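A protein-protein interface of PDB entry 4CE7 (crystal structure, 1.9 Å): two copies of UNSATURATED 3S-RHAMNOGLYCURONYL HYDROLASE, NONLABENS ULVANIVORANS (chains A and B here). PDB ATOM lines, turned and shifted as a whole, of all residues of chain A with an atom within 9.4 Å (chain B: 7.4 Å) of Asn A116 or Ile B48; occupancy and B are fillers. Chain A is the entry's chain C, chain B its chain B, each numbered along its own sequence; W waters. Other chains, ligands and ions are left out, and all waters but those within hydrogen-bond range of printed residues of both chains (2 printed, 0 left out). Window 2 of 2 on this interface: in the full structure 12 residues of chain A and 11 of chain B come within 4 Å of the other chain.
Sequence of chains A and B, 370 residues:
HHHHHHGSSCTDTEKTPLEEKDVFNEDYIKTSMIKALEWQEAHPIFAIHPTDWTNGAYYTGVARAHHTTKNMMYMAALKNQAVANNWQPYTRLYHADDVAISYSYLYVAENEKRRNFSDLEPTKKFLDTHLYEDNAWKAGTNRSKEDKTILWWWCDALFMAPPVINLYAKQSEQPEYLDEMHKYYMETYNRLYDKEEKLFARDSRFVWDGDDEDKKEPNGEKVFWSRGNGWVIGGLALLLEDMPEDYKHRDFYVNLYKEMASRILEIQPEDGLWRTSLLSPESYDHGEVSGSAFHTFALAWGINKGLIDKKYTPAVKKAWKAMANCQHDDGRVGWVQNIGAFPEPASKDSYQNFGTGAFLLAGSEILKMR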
ATOM      1  N   LYS A  79      -9.012  28.241 -28.097  1.00  0.00           N
ATOM      2  CA  LYS A  79      -9.485  26.885 -27.828  1.00  0.00           C
ATOM      3  C   LYS A  79      -9.084  26.002 -29.030  1.00  0.00           C
ATOM      4  O   LYS A  79      -8.632  24.864 -28.847  1.00  0.00           O
ATOM      5  CB  LYS A  79     -11.013  26.821 -27.580  1.00  0.00           C
ATOM      6  CG  LYS A  79     -11.355  27.449 -26.235  1.00  0.00           C
ATOM      7  CD  LYS A  79     -12.863  27.761 -26.144  1.00  0.00           C
ATOM      8  CE  LYS A  79     -13.668  26.471 -26.273  1.00  0.00           C
ATOM      9  NZ  LYS A  79     -15.102  26.750 -26.119  1.00  0.00           N
ATOM     10  N   ASN A  80      -9.331  26.463 -30.260  1.00  0.00           N
ATOM     11  CA  ASN A  80      -9.003  25.668 -31.468  1.00  0.00           C
ATOM     12  C   ASN A  80      -7.565  25.113 -31.426  1.00  0.00           C
ATOM     13  O   ASN A  80      -7.302  23.898 -31.642  1.00  0.00           O
ATOM     14  CB  ASN A  80      -9.145  26.566 -32.710  1.00  0.00           C
ATOM     15  CG  ASN A  80      -9.178  25.793 -34.038  1.00  0.00           C
ATOM     16  OD1 ASN A  80      -9.904  24.815 -34.198  1.00  0.00           O
ATOM     17  ND2 ASN A  80      -8.473  26.308 -35.017  1.00  0.00           N
ATOM     18  N   ALA A  82      -5.388  24.991 -28.938  1.00  0.00           N
ATOM     19  CA  ALA A  82      -5.039  24.192 -27.725  1.00  0.00           C
ATOM     20  C   ALA A  82      -5.520  22.748 -27.891  1.00  0.00           C
ATOM     21  O   ALA A  82      -4.810  21.800 -27.583  1.00  0.00           O
ATOM     22  CB  ALA A  82      -5.676  24.805 -26.481  1.00  0.00           C
ATOM     23  N   VAL A  83      -6.698  22.573 -28.472  1.00  0.00           N
ATOM     24  CA  VAL A  83      -7.175  21.191 -28.746  1.00  0.00           C
ATOM     25  C   VAL A  83      -6.394  20.603 -29.916  1.00  0.00           C
ATOM     26  O   VAL A  83      -6.002  19.453 -29.869  1.00  0.00           O
ATOM     27  CB  VAL A  83      -8.728  21.166 -29.043  1.00  0.00           C
ATOM     28  CG1 VAL A  83      -9.207  19.774 -29.525  1.00  0.00           C
ATOM     29  CG2 VAL A  83      -9.499  21.539 -27.748  1.00  0.00           C
ATOM     30  N   ALA A  84      -6.109  21.379 -30.947  1.00  0.00           N
ATOM     31  CA  ALA A  84      -5.369  20.820 -32.128  1.00  0.00           C
ATOM     32  C   ALA A  84      -3.973  20.342 -31.635  1.00  0.00           C
ATOM     33  O   ALA A  84      -3.433  19.295 -32.099  1.00  0.00           O
ATOM     34  CB  ALA A  84      -5.175  21.878 -33.246  1.00  0.00           C
ATOM     35  N   TRP A  87      -2.823  20.365 -26.010  1.00  0.00           N
ATOM     36  CA  TRP A  87      -2.387  21.029 -24.779  1.00  0.00           C
ATOM     37  C   TRP A  87      -0.910  20.770 -24.532  1.00  0.00           C
ATOM     38  O   TRP A  87      -0.418  20.876 -23.413  1.00  0.00           O
ATOM     39  CB  TRP A  87      -3.242  20.544 -23.577  1.00  0.00           C
ATOM     40  CG  TRP A  87      -4.749  20.821 -23.826  1.00  0.00           C
ATOM     41  CD1 TRP A  87      -5.693  19.980 -24.433  1.00  0.00           C
ATOM     42  CD2 TRP A  87      -5.461  22.076 -23.545  1.00  0.00           C
ATOM     43  NE1 TRP A  87      -6.944  20.606 -24.512  1.00  0.00           N
ATOM     44  CE2 TRP A  87      -6.870  21.874 -23.995  1.00  0.00           C
ATOM     45  CE3 TRP A  87      -5.099  23.306 -22.956  1.00  0.00           C
ATOM     46  CZ2 TRP A  87      -7.849  22.872 -23.850  1.00  0.00           C
ATOM     47  CZ3 TRP A  87      -6.098  24.305 -22.833  1.00  0.00           C
ATOM     48  CH2 TRP A  87      -7.423  24.093 -23.284  1.00  0.00           C
ATOM     49  N   VAL A 108      -6.573  29.923 -21.282  1.00  0.00           N
ATOM     50  CA  VAL A 108      -7.826  29.184 -21.576  1.00  0.00           C
ATOM     51  C   VAL A 108      -8.350  28.434 -20.368  1.00  0.00           C
ATOM     52  O   VAL A 108      -9.568  28.503 -20.054  1.00  0.00           O
ATOM     53  CB  VAL A 108      -7.656  28.246 -22.790  1.00  0.00           C
ATOM     54  CG1 VAL A 108      -8.977  27.471 -23.045  1.00  0.00           C
ATOM     55  CG2 VAL A 108      -7.363  29.165 -24.016  1.00  0.00           C
ATOM     56  N   GLU A 112     -11.945  29.826 -19.580  1.00  0.00           N
ATOM     57  CA  GLU A 112     -13.006  29.013 -20.159  1.00  0.00           C
ATOM     58  C   GLU A 112     -13.378  28.102 -19.019  1.00  0.00           C
ATOM     59  O   GLU A 112     -12.662  27.185 -18.678  1.00  0.00           O
ATOM     60  CB  GLU A 112     -12.490  28.206 -21.371  1.00  0.00           C
ATOM     61  CG  GLU A 112     -13.464  27.192 -21.952  1.00  0.00           C
ATOM     62  CD  GLU A 112     -14.502  27.824 -22.890  1.00  0.00           C
ATOM     63  OE1 GLU A 112     -14.468  29.041 -23.181  1.00  0.00           O
ATOM     64  OE2 GLU A 112     -15.346  27.090 -23.386  1.00  0.00           O
ATOM     65  N   LYS A 113     -14.509  28.398 -18.396  1.00  0.00           N
ATOM     66  CA  LYS A 113     -14.993  27.665 -17.241  1.00  0.00           C
ATOM     67  C   LYS A 113     -15.657  26.439 -17.785  1.00  0.00           C
ATOM     68  O   LYS A 113     -16.784  26.541 -18.237  1.00  0.00           O
ATOM     69  CB  LYS A 113     -16.067  28.525 -16.546  1.00  0.00           C
ATOM     70  CG  LYS A 113     -15.604  29.926 -16.209  1.00  0.00           C
ATOM     71  CD  LYS A 113     -14.716  29.792 -14.986  1.00  0.00           C
ATOM     72  CE  LYS A 113     -13.798  30.982 -14.828  1.00  0.00           C
ATOM     73  NZ  LYS A 113     -12.656  30.607 -13.947  1.00  0.00           N
ATOM     74  N   ARG A 114     -14.985  25.287 -17.772  1.00  0.00           N
ATOM     75  CA  ARG A 114     -15.547  24.111 -18.442  1.00  0.00           C
ATOM     76  C   ARG A 114     -14.797  22.884 -17.982  1.00  0.00           C
ATOM     77  O   ARG A 114     -13.556  22.851 -18.019  1.00  0.00           O
ATOM     78  CB  ARG A 114     -15.433  24.288 -19.960  1.00  0.00           C
ATOM     79  CG  ARG A 114     -16.043  23.223 -20.814  1.00  0.00           C
ATOM     80  CD  ARG A 114     -15.714  23.509 -22.286  1.00  0.00           C
ATOM     81  NE  ARG A 114     -16.373  24.739 -22.741  1.00  0.00           N
ATOM     82  CZ  ARG A 114     -17.688  24.848 -23.005  1.00  0.00           C
ATOM     83  NH1 ARG A 114     -18.528  23.805 -22.881  1.00  0.00           N
ATOM     84  NH2 ARG A 114     -18.170  26.020 -23.410  1.00  0.00           N
ATOM     85  N   ARG A 115     -15.540  21.862 -17.568  1.00  0.00           N
ATOM     86  CA  ARG A 115     -14.922  20.633 -17.075  1.00  0.00           C
ATOM     87  C   ARG A 115     -14.437  19.708 -18.159  1.00  0.00           C
ATOM     88  O   ARG A 115     -15.026  19.649 -19.263  1.00  0.00           O
ATOM     89  CB  ARG A 115     -15.929  19.838 -16.274  1.00  0.00           C
ATOM     90  CG  ARG A 115     -16.407  20.636 -15.102  1.00  0.00           C
ATOM     91  CD  ARG A 115     -16.178  19.910 -13.797  1.00  0.00           C
ATOM     92  NE  ARG A 115     -16.679  20.794 -12.741  1.00  0.00           N
ATOM     93  CZ  ARG A 115     -15.945  21.397 -11.801  1.00  0.00           C
ATOM     94  NH1 ARG A 115     -14.631  21.184 -11.738  1.00  0.00           N
ATOM     95  NH2 ARG A 115     -16.560  22.193 -10.898  1.00  0.00           N
ATOM     96  N   ASN A 116     -13.431  18.920 -17.788  1.00  0.00           N
ATOM     97  CA  ASN A 116     -12.864  17.898 -18.643  1.00  0.00           C
ATOM     98  C   ASN A 116     -12.554  18.471 -20.034  1.00  0.00           C
ATOM     99  O   ASN A 116     -12.892  17.856 -21.072  1.00  0.00           O
ATOM    100  CB  ASN A 116     -13.792  16.704 -18.763  1.00  0.00           C
ATOM    101  CG  ASN A 116     -14.119  16.098 -17.417  1.00  0.00           C
ATOM    102  OD1 ASN A 116     -15.285  15.946 -17.044  1.00  0.00           O
ATOM    103  ND2 ASN A 116     -13.096  15.796 -16.670  1.00  0.00           N
ATOM    104  N   PHE A 117     -11.939  19.639 -20.035  1.00  0.00           N
ATOM    105  CA  PHE A 117     -11.624  20.332 -21.285  1.00  0.00           C
ATOM    106  C   PHE A 117     -10.134  20.675 -21.302  1.00  0.00           C
ATOM    107  O   PHE A 117      -9.354  20.079 -22.051  1.00  0.00           O
ATOM    108  CB  PHE A 117     -12.500  21.597 -21.453  1.00  0.00           C
ATOM    109  CG  PHE A 117     -12.115  22.390 -22.646  1.00  0.00           C
ATOM    110  CD1 PHE A 117     -12.215  21.823 -23.908  1.00  0.00           C
ATOM    111  CD2 PHE A 117     -11.602  23.667 -22.512  1.00  0.00           C
ATOM    112  CE1 PHE A 117     -11.778  22.532 -25.047  1.00  0.00           C
ATOM    113  CE2 PHE A 117     -11.136  24.390 -23.622  1.00  0.00           C
ATOM    114  CZ  PHE A 117     -11.243  23.835 -24.901  1.00  0.00           C
ATOM    115  N   SER A 118      -9.714  21.628 -20.458  1.00  0.00           N
ATOM    116  CA  SER A 118      -8.312  22.043 -20.447  1.00  0.00           C
ATOM    117  C   SER A 118      -7.390  21.014 -19.758  1.00  0.00           C
ATOM    118  O   SER A 118      -7.821  20.246 -18.872  1.00  0.00           O
ATOM    119  CB  SER A 118      -8.180  23.435 -19.783  1.00  0.00           C
ATOM    120  OG  SER A 118      -8.646  23.365 -18.451  1.00  0.00           O
ATOM    121  N   ASP A 119      -6.136  20.927 -20.217  1.00  0.00           N
ATOM    122  CA  ASP A 119      -5.237  20.024 -19.581  1.00  0.00           C
ATOM    123  C   ASP A 119      -3.905  20.783 -19.346  1.00  0.00           C
ATOM    124  O   ASP A 119      -3.238  21.284 -20.282  1.00  0.00           O
ATOM    125  CB  ASP A 119      -5.108  18.744 -20.426  1.00  0.00           C
ATOM    126  CG  ASP A 119      -4.070  17.782 -19.884  1.00  0.00           C
ATOM    127  OD1 ASP A 119      -3.680  17.877 -18.697  1.00  0.00           O
ATOM    128  OD2 ASP A 119      -3.599  16.946 -20.670  1.00  0.00           O
ATOM    129  N   ILE B  45     -15.083  26.804 -34.639  1.00  0.00           N
ATOM    130  CA  ILE B  45     -15.433  27.075 -33.263  1.00  0.00           C
ATOM    131  C   ILE B  45     -16.113  25.765 -32.738  1.00  0.00           C
ATOM    132  O   ILE B  45     -16.615  24.963 -33.527  1.00  0.00           O
ATOM    133  CB  ILE B  45     -16.375  28.307 -33.131  1.00  0.00           C
ATOM    134  CG1 ILE B  45     -16.631  28.712 -31.632  1.00  0.00           C
ATOM    135  CG2 ILE B  45     -17.710  28.083 -33.926  1.00  0.00           C
ATOM    136  CD1 ILE B  45     -17.279  30.125 -31.523  1.00  0.00           C
ATOM    137  N   PHE B  46     -16.055  25.561 -31.434  1.00  0.00           N
ATOM    138  CA  PHE B  46     -16.748  24.442 -30.791  1.00  0.00           C
ATOM    139  C   PHE B  46     -16.938  24.818 -29.337  1.00  0.00           C
ATOM    140  O   PHE B  46     -16.233  25.707 -28.819  1.00  0.00           O
ATOM    141  CB  PHE B  46     -15.886  23.168 -30.876  1.00  0.00           C
ATOM    142  CG  PHE B  46     -14.430  23.347 -30.477  1.00  0.00           C
ATOM    143  CD1 PHE B  46     -14.046  23.372 -29.141  1.00  0.00           C
ATOM    144  CD2 PHE B  46     -13.412  23.338 -31.457  1.00  0.00           C
ATOM    145  CE1 PHE B  46     -12.698  23.528 -28.773  1.00  0.00           C
ATOM    146  CE2 PHE B  46     -12.061  23.444 -31.079  1.00  0.00           C
ATOM    147  CZ  PHE B  46     -11.718  23.518 -29.752  1.00  0.00           C
ATOM    148  N   ALA B  47     -17.892  24.173 -28.668  1.00  0.00           N
ATOM    149  CA  ALA B  47     -18.045  24.358 -27.228  1.00  0.00           C
ATOM    150  C   ALA B  47     -16.946  23.542 -26.513  1.00  0.00           C
ATOM    151  O   ALA B  47     -16.179  24.060 -25.704  1.00  0.00           O
ATOM    152  CB  ALA B  47     -19.444  23.850 -26.788  1.00  0.00           C
ATOM    153  N   ILE B  48     -16.837  22.267 -26.835  1.00  0.00           N
ATOM    154  CA  ILE B  48     -15.839  21.445 -26.138  1.00  0.00           C
ATOM    155  C   ILE B  48     -14.935  20.692 -27.097  1.00  0.00           C
ATOM    156  O   ILE B  48     -13.809  20.411 -26.744  1.00  0.00           O
ATOM    157  CB  ILE B  48     -16.530  20.398 -25.169  1.00  0.00           C
ATOM    158  CG1 ILE B  48     -15.464  19.645 -24.337  1.00  0.00           C
ATOM    159  CG2 ILE B  48     -17.398  19.415 -25.967  1.00  0.00           C
ATOM    160  CD1 ILE B  48     -15.910  19.195 -22.943  1.00  0.00           C
ATOM    161  N   HIS B  49     -15.413  20.376 -28.300  1.00  0.00           N
ATOM    162  CA  HIS B  49     -14.567  19.646 -29.282  1.00  0.00           C
ATOM    163  C   HIS B  49     -15.109  19.785 -30.706  1.00  0.00           C
ATOM    164  O   HIS B  49     -16.309  19.878 -30.873  1.00  0.00           O
ATOM    165  CB  HIS B  49     -14.554  18.161 -28.882  1.00  0.00           C
ATOM    166  CG  HIS B  49     -13.450  17.375 -29.541  1.00  0.00           C
ATOM    167  ND1 HIS B  49     -13.661  16.655 -30.671  1.00  0.00           N
ATOM    168  CD2 HIS B  49     -12.077  17.243 -29.229  1.00  0.00           C
ATOM    169  CE1 HIS B  49     -12.499  16.085 -31.091  1.00  0.00           C
ATOM    170  NE2 HIS B  49     -11.522  16.429 -30.189  1.00  0.00           N
ATOM    171  N   PRO B  50     -14.236  19.733 -31.747  1.00  0.00           N
ATOM    172  CA  PRO B  50     -14.705  19.800 -33.160  1.00  0.00           C
ATOM    173  C   PRO B  50     -15.813  18.760 -33.509  1.00  0.00           C
ATOM    174  O   PRO B  50     -16.598  18.970 -34.441  1.00  0.00           O
ATOM    175  CB  PRO B  50     -13.397  19.543 -33.993  1.00  0.00           C
ATOM    176  CG  PRO B  50     -12.327  20.091 -33.120  1.00  0.00           C
ATOM    177  CD  PRO B  50     -12.737  19.712 -31.666  1.00  0.00           C
ATOM    178  N   THR B  51     -15.884  17.688 -32.753  1.00  0.00           N
ATOM    179  CA  THR B  51     -16.894  16.690 -32.992  1.00  0.00           C
ATOM    180  C   THR B  51     -18.170  16.889 -32.143  1.00  0.00           C
ATOM    181  O   THR B  51     -19.001  16.060 -32.082  1.00  0.00           O
ATOM    182  CB  THR B  51     -16.385  15.284 -32.782  1.00  0.00           C
ATOM    183  OG1 THR B  51     -16.010  15.075 -31.423  1.00  0.00           O
ATOM    184  CG2 THR B  51     -15.311  14.895 -33.768  1.00  0.00           C
ATOM    185  N   ASP B  52     -18.287  18.008 -31.486  1.00  0.00           N
ATOM    186  CA  ASP B  52     -19.424  18.221 -30.521  1.00  0.00           C
ATOM    187  C   ASP B  52     -20.702  18.647 -31.228  1.00  0.00           C
ATOM    188  O   ASP B  52     -20.668  18.877 -32.473  1.00  0.00           O
ATOM    189  CB  ASP B  52     -19.073  19.193 -29.389  1.00  0.00           C
ATOM    190  CG  ASP B  52     -18.916  20.688 -29.857  1.00  0.00           C
ATOM    191  OD1 ASP B  52     -19.414  21.083 -30.943  1.00  0.00           O
ATOM    192  OD2 ASP B  52     -18.335  21.473 -29.068  1.00  0.00           O
ATOM    193  N   TRP B  53     -21.825  18.833 -30.484  1.00  0.00           N
ATOM    194  CA  TRP B  53     -23.131  19.115 -31.122  1.00  0.00           C
ATOM    195  C   TRP B  53     -23.151  20.416 -31.940  1.00  0.00           C
ATOM    196  O   TRP B  53     -23.929  20.543 -32.895  1.00  0.00           O
ATOM    197  CB  TRP B  53     -24.282  19.125 -30.073  1.00  0.00           C
ATOM    198  CG  TRP B  53     -24.158  20.294 -29.110  1.00  0.00           C
ATOM    199  CD1 TRP B  53     -23.461  20.341 -27.884  1.00  0.00           C
ATOM    200  CD2 TRP B  53     -24.718  21.614 -29.272  1.00  0.00           C
ATOM    201  NE1 TRP B  53     -23.576  21.570 -27.330  1.00  0.00           N
ATOM    202  CE2 TRP B  53     -24.336  22.368 -28.089  1.00  0.00           C
ATOM    203  CE3 TRP B  53     -25.401  22.256 -30.301  1.00  0.00           C
ATOM    204  CZ2 TRP B  53     -24.670  23.708 -27.926  1.00  0.00           C
ATOM    205  CZ3 TRP B  53     -25.789  23.582 -30.113  1.00  0.00           C
ATOM    206  CH2 TRP B  53     -25.426  24.295 -28.951  1.00  0.00           C
ATOM    207  N   THR B  54     -22.284  21.385 -31.601  1.00  0.00           N
ATOM    208  CA  THR B  54     -22.285  22.700 -32.249  1.00  0.00           C
ATOM    209  C   THR B  54     -21.830  22.463 -33.694  1.00  0.00           C
ATOM    210  O   THR B  54     -22.461  22.992 -34.647  1.00  0.00           O
ATOM    211  CB  THR B  54     -21.472  23.794 -31.509  1.00  0.00           C
ATOM    212  OG1 THR B  54     -20.032  23.580 -31.637  1.00  0.00           O
ATOM    213  CG2 THR B  54     -21.904  23.922 -30.008  1.00  0.00           C
ATOM    214  N   ASN B  55     -20.816  21.605 -33.874  1.00  0.00           N
ATOM    215  CA  ASN B  55     -20.359  21.330 -35.251  1.00  0.00           C
ATOM    216  C   ASN B  55     -21.297  20.338 -35.942  1.00  0.00           C
ATOM    217  O   ASN B  55     -21.407  20.360 -37.150  1.00  0.00           O
ATOM    218  CB  ASN B  55     -18.908  20.829 -35.276  1.00  0.00           C
ATOM    219  CG  ASN B  55     -17.943  21.963 -35.041  1.00  0.00           C
ATOM    220  OD1 ASN B  55     -17.722  22.777 -35.960  1.00  0.00           O
ATOM    221  ND2 ASN B  55     -17.613  22.201 -33.754  1.00  0.00           N
ATOM    222  N   TYR B  90     -18.316  12.403 -30.640  1.00  0.00           N
ATOM    223  CA  TYR B  90     -17.653  12.735 -29.381  1.00  0.00           C
ATOM    224  C   TYR B  90     -17.916  11.558 -28.381  1.00  0.00           C
ATOM    225  O   TYR B  90     -18.524  10.545 -28.758  1.00  0.00           O
ATOM    226  CB  TYR B  90     -18.047  14.129 -28.886  1.00  0.00           C
ATOM    227  CG  TYR B  90     -17.084  14.640 -27.797  1.00  0.00           C
ATOM    228  CD1 TYR B  90     -15.677  14.688 -28.031  1.00  0.00           C
ATOM    229  CD2 TYR B  90     -17.579  15.143 -26.600  1.00  0.00           C
ATOM    230  CE1 TYR B  90     -14.781  15.150 -27.061  1.00  0.00           C
ATOM    231  CE2 TYR B  90     -16.712  15.646 -25.647  1.00  0.00           C
ATOM    232  CZ  TYR B  90     -15.332  15.599 -25.842  1.00  0.00           C
ATOM    233  OH  TYR B  90     -14.486  16.099 -24.862  1.00  0.00           O
ATOM    234  N   ARG B  92     -19.083  10.943 -25.006  1.00  0.00           N
ATOM    235  CA  ARG B  92     -19.998  10.657 -23.872  1.00  0.00           C
ATOM    236  C   ARG B  92     -21.131   9.876 -24.474  1.00  0.00           C
ATOM    237  O   ARG B  92     -22.069  10.443 -25.049  1.00  0.00           O
ATOM    238  CB  ARG B  92     -20.472  11.909 -23.132  1.00  0.00           C
ATOM    239  CG  ARG B  92     -19.306  12.628 -22.444  1.00  0.00           C
ATOM    240  CD  ARG B  92     -19.668  14.064 -22.176  1.00  0.00           C
ATOM    241  NE  ARG B  92     -20.118  14.720 -23.409  1.00  0.00           N
ATOM    242  CZ  ARG B  92     -20.622  15.948 -23.448  1.00  0.00           C
ATOM    243  NH1 ARG B  92     -20.706  16.614 -22.304  1.00  0.00           N
ATOM    244  NH2 ARG B  92     -21.044  16.531 -24.585  1.00  0.00           N
ATOM    245  N   ASP B  98     -23.465  14.203 -28.342  1.00  0.00           N
ATOM    246  CA  ASP B  98     -22.184  13.718 -28.844  1.00  0.00           C
ATOM    247  C   ASP B  98     -22.270  12.964 -30.201  1.00  0.00           C
ATOM    248  O   ASP B  98     -21.241  12.628 -30.827  1.00  0.00           O
ATOM    249  CB  ASP B  98     -21.471  12.917 -27.743  1.00  0.00           C
ATOM    250  CG  ASP B  98     -20.861  13.812 -26.704  1.00  0.00           C
ATOM    251  OD1 ASP B  98     -21.094  15.071 -26.756  1.00  0.00           O
ATOM    252  OD2 ASP B  98     -20.156  13.236 -25.816  1.00  0.00           O
ATOM    253  N   ILE B 339     -24.589  29.972 -26.887  1.00  0.00           N
ATOM    254  CA  ILE B 339     -25.047  28.672 -26.455  1.00  0.00           C
ATOM    255  C   ILE B 339     -25.871  28.901 -25.168  1.00  0.00           C
ATOM    256  O   ILE B 339     -25.499  29.746 -24.341  1.00  0.00           O
ATOM    257  CB  ILE B 339     -23.826  27.792 -26.153  1.00  0.00           C
ATOM    258  CG1 ILE B 339     -23.191  27.316 -27.480  1.00  0.00           C
ATOM    259  CG2 ILE B 339     -24.200  26.554 -25.299  1.00  0.00           C
ATOM    260  CD1 ILE B 339     -21.826  26.696 -27.288  1.00  0.00           C
HETATM  261  O   HOH W   1     -15.617  28.614 -28.276  1.00  0.00           O
HETATM  262  O   HOH W   2     -14.998  16.348 -22.312  1.00  0.00           O
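The backbone carbonyl oxygen of Ala B47 sits at hydrogen-bond distance from the guanidinium group of Arg A114, 3.0 Å away. NZ of Lys A79 is in hydrogen-bond range of O of Ala B47, 2.9 Å away. O of Phe B46 sits at hydrogen-bond distance from NZ of Lys A79 (3.1 Å).
The side-chain carboxylate (OE2) of Glu A112 lies within salt-bridge range of the guanidinium group (NE) of Arg A114, at 2.6 Å. O of Phe A117 sits at hydrogen-bond distance from NE1 of Trp A87 (3.5 Å). OD2 of Asp B52 lies within hydrogen-bond range of N of His B49 (3.2 Å). The side-chain amino group (NZ) of Lys A79 lies within salt-bridge range of the side-chain carboxylate (OE2) of Glu A112 (2.8 Å). The backbone NH of Ala B47 lies within hydrogen-bond range of the side-chain carboxylate of Asp B52, at 2.8 Å. The backbone NH (N) of Ile B48 sits at hydrogen-bond distance from the side-chain carboxylate (OD2) of Asp B52, 2.8 Å away.
CE2 of Phe B46 touches CA of Asn A80, 3.8 Å away. Phe B46 touches Val A83 (CZ to CG2, 3.6 Å). CG1 of Val A83 touches CD2 of His B49 (3.8 Å). OE2 of Glu A112 touches O of Ala B47 (3.9 Å). Ile B48 touches Arg A115. Asn A116 touches Ile B48 (O to CD1, 3.8 Å). Phe A117 touches Phe B46 (CE1 to CE1, 3.97 Å). Phe A117 touches Ile B48 (CE1 to O, 3.4 Å).
Of the printed residues of chain B, Asn A116 touches Ile B48. Ile B48 touches just these residues of chain A: Arg A115 (3.8 Å), Asn A116 (3.8 Å) and Phe A117 (3.4 Å). Of chain A, only Lys A79 (2.9 Å), Glu A112 (3.9 Å) and Arg A114 (3.0 Å) come within 4 Å of Ala B47. Of the printed residues of chain B, Asn A80 touches Phe B46. Printed residues of chain B within 4 Å of Arg A114: Ala B47 (3.0 Å). Of the printed residues of chain B, Lys A79 touches Phe B46 (3.1 Å) and Ala B47 (2.9 Å). Of the printed residues of chain B, Glu A112 touches Ala B47 (3.9 Å). Of the printed residues of chain B, Val A83 touches Phe B46 and His B49. Ala A82 touches none of the printed residues of chain B. The nearest residue of chain A that does not touch Ile B48 is Arg A114 (4.3 Å).
Of the 15 printed residues of chain B, 4 touch a printed residue of chain A. Printed residues of chain A that touch a printed residue of chain B: Lys A79, Asn A80, Val A83, Glu A112, Arg A114, Arg A115, Asn A116 and Phe A117. Hydrophobic or aromatic side chains of chain A within 4 Å of the printed part of chain B: Val A83 and Phe A117. Among the printed residues, 11 pairs touch across the chains. Among the printed residues, no Asp or Glu carboxylate lies within 4 Å of a Lys or Arg side-chain nitrogen of the other chain.
No position is printed for both chains. Of the 11 pairs that touch across the chains among the printed residues, none has its exchanged pair printed and touching as well.
Water W2 bridges OH of Tyr B90 and O of Asn A116. Water W1 lies within hydrogen-bond range of NZ of Lys A79 and O of Phe B46.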
